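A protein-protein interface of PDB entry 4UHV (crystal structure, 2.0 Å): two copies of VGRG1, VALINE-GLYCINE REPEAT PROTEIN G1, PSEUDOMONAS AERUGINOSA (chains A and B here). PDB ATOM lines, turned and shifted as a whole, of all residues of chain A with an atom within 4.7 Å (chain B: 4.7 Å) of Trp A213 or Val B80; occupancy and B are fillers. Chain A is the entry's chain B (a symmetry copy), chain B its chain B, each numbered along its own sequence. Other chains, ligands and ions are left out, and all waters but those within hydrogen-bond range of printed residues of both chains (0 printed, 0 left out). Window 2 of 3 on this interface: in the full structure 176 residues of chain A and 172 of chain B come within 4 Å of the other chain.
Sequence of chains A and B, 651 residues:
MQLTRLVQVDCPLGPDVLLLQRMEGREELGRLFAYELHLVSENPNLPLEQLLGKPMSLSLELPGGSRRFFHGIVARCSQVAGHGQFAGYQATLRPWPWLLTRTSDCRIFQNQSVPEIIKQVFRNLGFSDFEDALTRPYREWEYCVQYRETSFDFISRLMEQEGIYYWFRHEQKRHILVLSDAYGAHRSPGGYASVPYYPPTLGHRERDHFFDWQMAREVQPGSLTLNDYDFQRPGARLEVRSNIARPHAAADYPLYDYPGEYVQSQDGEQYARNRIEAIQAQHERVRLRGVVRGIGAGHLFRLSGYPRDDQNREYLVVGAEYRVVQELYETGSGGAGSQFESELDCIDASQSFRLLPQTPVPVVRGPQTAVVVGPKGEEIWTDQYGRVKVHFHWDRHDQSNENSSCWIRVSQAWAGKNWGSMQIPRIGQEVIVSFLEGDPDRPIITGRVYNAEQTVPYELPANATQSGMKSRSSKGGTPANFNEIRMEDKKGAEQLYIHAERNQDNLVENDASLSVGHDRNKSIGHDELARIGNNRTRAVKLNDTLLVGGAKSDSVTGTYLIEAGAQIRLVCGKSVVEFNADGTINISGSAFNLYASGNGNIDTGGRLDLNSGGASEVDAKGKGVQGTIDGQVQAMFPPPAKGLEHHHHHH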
ATOM      1  N   TYR A 197       0.034 -16.419   9.954  1.00  0.00           N
ATOM      2  CA  TYR A 197       0.764 -16.593   8.704  1.00  0.00           C
ATOM      3  C   TYR A 197       0.757 -18.090   8.361  1.00  0.00           C
ATOM      4  O   TYR A 197       1.104 -18.928   9.196  1.00  0.00           O
ATOM      5  CB  TYR A 197       2.185 -16.061   8.864  1.00  0.00           C
ATOM      6  CG  TYR A 197       2.991 -15.925   7.591  1.00  0.00           C
ATOM      7  CD1 TYR A 197       3.518 -17.039   6.952  1.00  0.00           C
ATOM      8  CD2 TYR A 197       3.275 -14.674   7.057  1.00  0.00           C
ATOM      9  CE1 TYR A 197       4.276 -16.909   5.796  1.00  0.00           C
ATOM     10  CE2 TYR A 197       4.033 -14.533   5.906  1.00  0.00           C
ATOM     11  CZ  TYR A 197       4.530 -15.651   5.277  1.00  0.00           C
ATOM     12  OH  TYR A 197       5.287 -15.506   4.133  1.00  0.00           O
ATOM     13  N   ASP A 212       2.583 -14.565   2.160  1.00  0.00           N
ATOM     14  CA  ASP A 212       3.671 -13.966   1.371  1.00  0.00           C
ATOM     15  C   ASP A 212       4.578 -13.081   2.238  1.00  0.00           C
ATOM     16  O   ASP A 212       4.083 -12.340   3.082  1.00  0.00           O
ATOM     17  CB  ASP A 212       3.097 -13.125   0.226  1.00  0.00           C
ATOM     18  CG  ASP A 212       4.158 -12.325  -0.508  1.00  0.00           C
ATOM     19  OD1 ASP A 212       5.311 -12.799  -0.621  1.00  0.00           O
ATOM     20  OD2 ASP A 212       3.831 -11.216  -0.975  1.00  0.00           O
ATOM     21  N   TRP A 213       5.892 -13.155   2.023  1.00  0.00           N
ATOM     22  CA  TRP A 213       6.845 -12.173   2.583  1.00  0.00           C
ATOM     23  C   TRP A 213       7.935 -11.845   1.567  1.00  0.00           C
ATOM     24  O   TRP A 213       8.293 -12.673   0.744  1.00  0.00           O
ATOM     25  CB  TRP A 213       7.440 -12.690   3.904  1.00  0.00           C
ATOM     26  CG  TRP A 213       8.776 -12.067   4.403  1.00  0.00           C
ATOM     27  CD1 TRP A 213       8.929 -11.194   5.443  1.00  0.00           C
ATOM     28  CD2 TRP A 213      10.099 -12.325   3.913  1.00  0.00           C
ATOM     29  NE1 TRP A 213      10.254 -10.877   5.618  1.00  0.00           N
ATOM     30  CE2 TRP A 213      10.994 -11.560   4.693  1.00  0.00           C
ATOM     31  CE3 TRP A 213      10.617 -13.109   2.878  1.00  0.00           C
ATOM     32  CZ2 TRP A 213      12.369 -11.575   4.478  1.00  0.00           C
ATOM     33  CZ3 TRP A 213      11.977 -13.110   2.660  1.00  0.00           C
ATOM     34  CH2 TRP A 213      12.840 -12.345   3.459  1.00  0.00           C
ATOM     35  N   GLN A 214       8.441 -10.619   1.629  1.00  0.00           N
ATOM     36  CA  GLN A 214       9.593 -10.196   0.840  1.00  0.00           C
ATOM     37  C   GLN A 214      10.230  -9.047   1.605  1.00  0.00           C
ATOM     38  O   GLN A 214       9.532  -8.123   2.010  1.00  0.00           O
ATOM     39  CB  GLN A 214       9.162  -9.720  -0.545  1.00  0.00           C
ATOM     40  CG  GLN A 214      10.297  -9.635  -1.563  1.00  0.00           C
ATOM     41  CD  GLN A 214      10.051  -8.613  -2.671  1.00  0.00           C
ATOM     42  OE1 GLN A 214       8.915  -8.361  -3.052  1.00  0.00           O
ATOM     43  NE2 GLN A 214      11.122  -8.029  -3.193  1.00  0.00           N
ATOM     44  N   MET A 215      11.542  -9.103   1.803  1.00  0.00           N
ATOM     45  CA  MET A 215      12.268  -8.030   2.486  1.00  0.00           C
ATOM     46  C   MET A 215      13.236  -7.364   1.554  1.00  0.00           C
ATOM     47  O   MET A 215      14.384  -7.799   1.419  1.00  0.00           O
ATOM     48  CB  MET A 215      13.041  -8.612   3.658  1.00  0.00           C
ATOM     49  CG  MET A 215      13.985  -7.575   4.258  1.00  0.00           C
ATOM     50  SD  MET A 215      14.237  -7.982   6.155  1.00  0.00           S
ATOM     51  CE  MET A 215      15.895  -9.039   5.965  1.00  0.00           C
ATOM     52  N   VAL A 286       9.498  -3.952   3.966  1.00  0.00           N
ATOM     53  CA  VAL A 286       9.027  -5.349   3.840  1.00  0.00           C
ATOM     54  C   VAL A 286       7.652  -5.456   3.160  1.00  0.00           C
ATOM     55  O   VAL A 286       6.763  -4.650   3.405  1.00  0.00           O
ATOM     56  CB  VAL A 286       9.040  -6.075   5.214  1.00  0.00           C
ATOM     57  CG1 VAL A 286       8.486  -5.184   6.314  1.00  0.00           C
ATOM     58  CG2 VAL A 286       8.288  -7.406   5.172  1.00  0.00           C
ATOM     59  N   ARG A 287       7.489  -6.478   2.314  1.00  0.00           N
ATOM     60  CA  ARG A 287       6.346  -6.580   1.408  1.00  0.00           C
ATOM     61  C   ARG A 287       5.499  -7.820   1.698  1.00  0.00           C
ATOM     62  O   ARG A 287       6.002  -8.939   1.617  1.00  0.00           O
ATOM     63  CB  ARG A 287       6.854  -6.618  -0.030  1.00  0.00           C
ATOM     64  CG  ARG A 287       5.954  -5.937  -1.041  1.00  0.00           C
ATOM     65  CD  ARG A 287       6.105  -6.524  -2.432  1.00  0.00           C
ATOM     66  NE  ARG A 287       6.059  -7.995  -2.426  1.00  0.00           N
ATOM     67  CZ  ARG A 287       4.986  -8.743  -2.684  1.00  0.00           C
ATOM     68  NH1 ARG A 287       3.812  -8.200  -2.984  1.00  0.00           N
ATOM     69  NH2 ARG A 287       5.097 -10.064  -2.656  1.00  0.00           N
ATOM     70  N   LEU A 288       4.221  -7.633   2.034  1.00  0.00           N
ATOM     71  CA  LEU A 288       3.366  -8.780   2.416  1.00  0.00           C
ATOM     72  C   LEU A 288       2.023  -8.906   1.690  1.00  0.00           C
ATOM     73  O   LEU A 288       1.567  -8.020   0.973  1.00  0.00           O
ATOM     74  CB  LEU A 288       3.121  -8.777   3.919  1.00  0.00           C
ATOM     75  CG  LEU A 288       4.406  -8.597   4.728  1.00  0.00           C
ATOM     76  CD1 LEU A 288       4.481  -7.180   5.277  1.00  0.00           C
ATOM     77  CD2 LEU A 288       4.506  -9.635   5.832  1.00  0.00           C
ATOM     78  N   TYR A 306       6.088 -16.804   9.813  1.00  0.00           N
ATOM     79  CA  TYR A 306       7.444 -16.768   9.266  1.00  0.00           C
ATOM     80  C   TYR A 306       8.346 -16.237  10.366  1.00  0.00           C
ATOM     81  O   TYR A 306       8.418 -15.020  10.579  1.00  0.00           O
ATOM     82  CB  TYR A 306       7.565 -15.869   8.027  1.00  0.00           C
ATOM     83  CG  TYR A 306       8.923 -16.024   7.354  1.00  0.00           C
ATOM     84  CD1 TYR A 306      10.101 -15.706   8.031  1.00  0.00           C
ATOM     85  CD2 TYR A 306       9.033 -16.526   6.068  1.00  0.00           C
ATOM     86  CE1 TYR A 306      11.336 -15.871   7.442  1.00  0.00           C
ATOM     87  CE2 TYR A 306      10.268 -16.691   5.473  1.00  0.00           C
ATOM     88  CZ  TYR A 306      11.417 -16.365   6.165  1.00  0.00           C
ATOM     89  OH  TYR A 306      12.657 -16.528   5.588  1.00  0.00           O
ATOM     90  N   GLN A 311      13.911 -11.159  13.788  1.00  0.00           N
ATOM     91  CA  GLN A 311      13.700 -10.558  12.455  1.00  0.00           C
ATOM     92  C   GLN A 311      12.313  -9.945  12.417  1.00  0.00           C
ATOM     93  O   GLN A 311      12.135  -8.759  12.103  1.00  0.00           O
ATOM     94  CB  GLN A 311      13.796 -11.582  11.323  1.00  0.00           C
ATOM     95  CG  GLN A 311      13.495 -10.992   9.931  1.00  0.00           C
ATOM     96  CD  GLN A 311      12.749 -11.919   8.963  1.00  0.00           C
ATOM     97  OE1 GLN A 311      12.998 -11.886   7.761  1.00  0.00           O
ATOM     98  NE2 GLN A 311      11.816 -12.717   9.470  1.00  0.00           N
ATOM     99  N   SER B  78      16.890  -8.481  -2.357  1.00  0.00           N
ATOM    100  CA  SER B  78      15.803  -9.036  -1.571  1.00  0.00           C
ATOM    101  C   SER B  78      15.777 -10.540  -1.615  1.00  0.00           C
ATOM    102  O   SER B  78      16.370 -11.162  -2.500  1.00  0.00           O
ATOM    103  CB  SER B  78      14.464  -8.542  -2.102  1.00  0.00           C
ATOM    104  OG  SER B  78      13.400  -9.079  -1.330  1.00  0.00           O
ATOM    105  N   GLN B  79      15.070 -11.116  -0.647  1.00  0.00           N
ATOM    106  CA  GLN B  79      14.759 -12.555  -0.627  1.00  0.00           C
ATOM    107  C   GLN B  79      13.233 -12.669  -0.755  1.00  0.00           C
ATOM    108  O   GLN B  79      12.546 -11.653  -0.782  1.00  0.00           O
ATOM    109  CB  GLN B  79      15.279 -13.204   0.665  1.00  0.00           C
ATOM    110  CG  GLN B  79      15.555 -14.702   0.567  1.00  0.00           C
ATOM    111  CD  GLN B  79      16.369 -15.265   1.734  1.00  0.00           C
ATOM    112  OE1 GLN B  79      16.714 -14.554   2.678  1.00  0.00           O
ATOM    113  NE2 GLN B  79      16.675 -16.565   1.668  1.00  0.00           N
ATOM    114  N   VAL B  80      12.701 -13.884  -0.869  1.00  0.00           N
ATOM    115  CA  VAL B  80      11.259 -14.061  -1.022  1.00  0.00           C
ATOM    116  C   VAL B  80      10.769 -15.315  -0.298  1.00  0.00           C
ATOM    117  O   VAL B  80      11.320 -16.405  -0.478  1.00  0.00           O
ATOM    118  CB  VAL B  80      10.841 -14.141  -2.513  1.00  0.00           C
ATOM    119  CG1 VAL B  80       9.419 -13.620  -2.699  1.00  0.00           C
ATOM    120  CG2 VAL B  80      11.786 -13.346  -3.405  1.00  0.00           C
ATOM    121  N   ALA B  81       9.730 -15.148   0.517  1.00  0.00           N
ATOM    122  CA  ALA B  81       9.124 -16.248   1.254  1.00  0.00           C
ATOM    123  C   ALA B  81       7.874 -16.632   0.507  1.00  0.00           C
ATOM    124  O   ALA B  81       6.757 -16.251   0.882  1.00  0.00           O
ATOM    125  CB  ALA B  81       8.781 -15.844   2.674  1.00  0.00           C
ATOM    126  N   GLY B  82       8.090 -17.333  -0.597  1.00  0.00           N
ATOM    127  CA  GLY B  82       7.036 -18.033  -1.308  1.00  0.00           C
ATOM    128  C   GLY B  82       7.263 -19.517  -1.109  1.00  0.00           C
ATOM    129  O   GLY B  82       6.366 -20.249  -0.672  1.00  0.00           O
ATOM    130  N   HIS B  83       8.481 -19.948  -1.426  1.00  0.00           N
ATOM    131  CA  HIS B  83       8.886 -21.328  -1.269  1.00  0.00           C
ATOM    132  C   HIS B  83       9.859 -21.481  -0.105  1.00  0.00           C
ATOM    133  O   HIS B  83      10.912 -20.823  -0.061  1.00  0.00           O
ATOM    134  CB  HIS B  83       9.536 -21.817  -2.556  1.00  0.00           C
ATOM    135  CG  HIS B  83       8.585 -21.920  -3.705  1.00  0.00           C
ATOM    136  ND1 HIS B  83       8.478 -23.053  -4.480  1.00  0.00           N
ATOM    137  CD2 HIS B  83       7.689 -21.036  -4.202  1.00  0.00           C
ATOM    138  CE1 HIS B  83       7.556 -22.862  -5.407  1.00  0.00           C
ATOM    139  NE2 HIS B  83       7.064 -21.645  -5.262  1.00  0.00           N
ATOM    140  N   GLY B  88      14.270 -18.172  -2.959  1.00  0.00           N
ATOM    141  CA  GLY B  88      14.086 -17.294  -4.118  1.00  0.00           C
ATOM    142  C   GLY B  88      14.537 -15.884  -3.771  1.00  0.00           C
ATOM    143  O   GLY B  88      14.295 -15.422  -2.660  1.00  0.00           O
ATOM    144  N   TYR B  89      15.198 -15.198  -4.707  1.00  0.00           N
ATOM    145  CA  TYR B  89      15.693 -13.833  -4.456  1.00  0.00           C
ATOM    146  C   TYR B  89      15.425 -12.875  -5.629  1.00  0.00           C
ATOM    147  O   TYR B  89      14.979 -13.292  -6.712  1.00  0.00           O
ATOM    148  CB  TYR B  89      17.205 -13.829  -4.181  1.00  0.00           C
ATOM    149  CG  TYR B  89      17.736 -14.964  -3.330  1.00  0.00           C
ATOM    150  CD1 TYR B  89      17.881 -16.244  -3.856  1.00  0.00           C
ATOM    151  CD2 TYR B  89      18.116 -14.751  -2.008  1.00  0.00           C
ATOM    152  CE1 TYR B  89      18.373 -17.288  -3.092  1.00  0.00           C
ATOM    153  CE2 TYR B  89      18.605 -15.793  -1.230  1.00  0.00           C
ATOM    154  CZ  TYR B  89      18.729 -17.064  -1.781  1.00  0.00           C
ATOM    155  OH  TYR B  89      19.223 -18.107  -1.038  1.00  0.00           O
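The backbone NH of Val B80 is in hydrogen-bond range of the backbone carbonyl oxygen of Gly B88, at 2.8 Å. The side-chain hydroxyl (OH) of Tyr A197 lies close to the backbone NH (N) of Asp A212 (3.5 Å). The side-chain hydroxyl (OH) of Tyr A197 sits at hydrogen-bond distance from the backbone NH (N) of Trp A213 (3.2 Å). NH2 of Arg A287 is in salt-bridge range of OD1 of Asp A212 (3.4 Å). The backbone carbonyl oxygen of Gln A214 lies within hydrogen-bond range of the backbone NH of Arg A287, at 2.6 Å.
Of the 10 printed residues of chain A, 6 touch a printed residue of chain B. Hydrophobic or aromatic side chains of chain A within 4 Å of the printed part of chain B: Tyr A197, Trp A213 and Tyr A306. Printed residues of chain B that touch a printed residue of chain A: Ser B78, Gln B79, Val B80 and Ala B81. Hydrophobic or aromatic side chains of chain B within 4 Å of the printed part of chain A: Val B80 and Ala B81. Along chain B the printed residues that touch a printed residue of chain A span positions 78 to 81. Among the printed residues, 10 pairs touch across the chains.
Among the printed residues, merely in contact across the chains: Gln A214 with Gln B79, Tyr A306 with Ala B81, Tyr A197 with Ala B81, Trp A213 with Gln B79, Trp A213 with Val B80, Met A215 with Gln B79 and Asp A212 with Ala B81.
No position is printed for both chains. Of the 10 pairs that touch across the chains among the printed residues, none has its exchanged pair printed and touching as well.
Printed residues of chain B within 4 Å of Tyr A197: Ala B81 (3.6 Å). Of the printed residues of chain B, Asp A212 touches Ala B81 (3.9 Å). Of the printed residues of chain B, Trp A213 touches Gln B79, Val B80 and Ala B81. Of the printed residues of chain B, Met A215 touches Ser B78 (3.2 Å) and Gln B79 (3.8 Å). Printed residues of chain B within 4 Å of Tyr A306: Ala B81. Of the printed residues of chain A, Gln B79 touches Trp A213, Gln A214 and Met A215. His B83 touches none of the printed residues of chain A. The nearest printed residue of chain A that does not touch Ser B78 is Trp A213 (5.8 Å).
The side-chain amide nitrogen of Gln A214 sits at hydrogen-bond distance from the side-chain hydroxyl of Ser B78. The side-chain hydroxyl (OG) of Ser B78 lies within hydrogen-bond range of the backbone carbonyl oxygen (O) of Met A215, at 3.2 Å. The backbone NH (N) of Ala B81 lies within hydrogen-bond range of the backbone carbonyl oxygen (O) of Trp A213 (2.9 Å).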
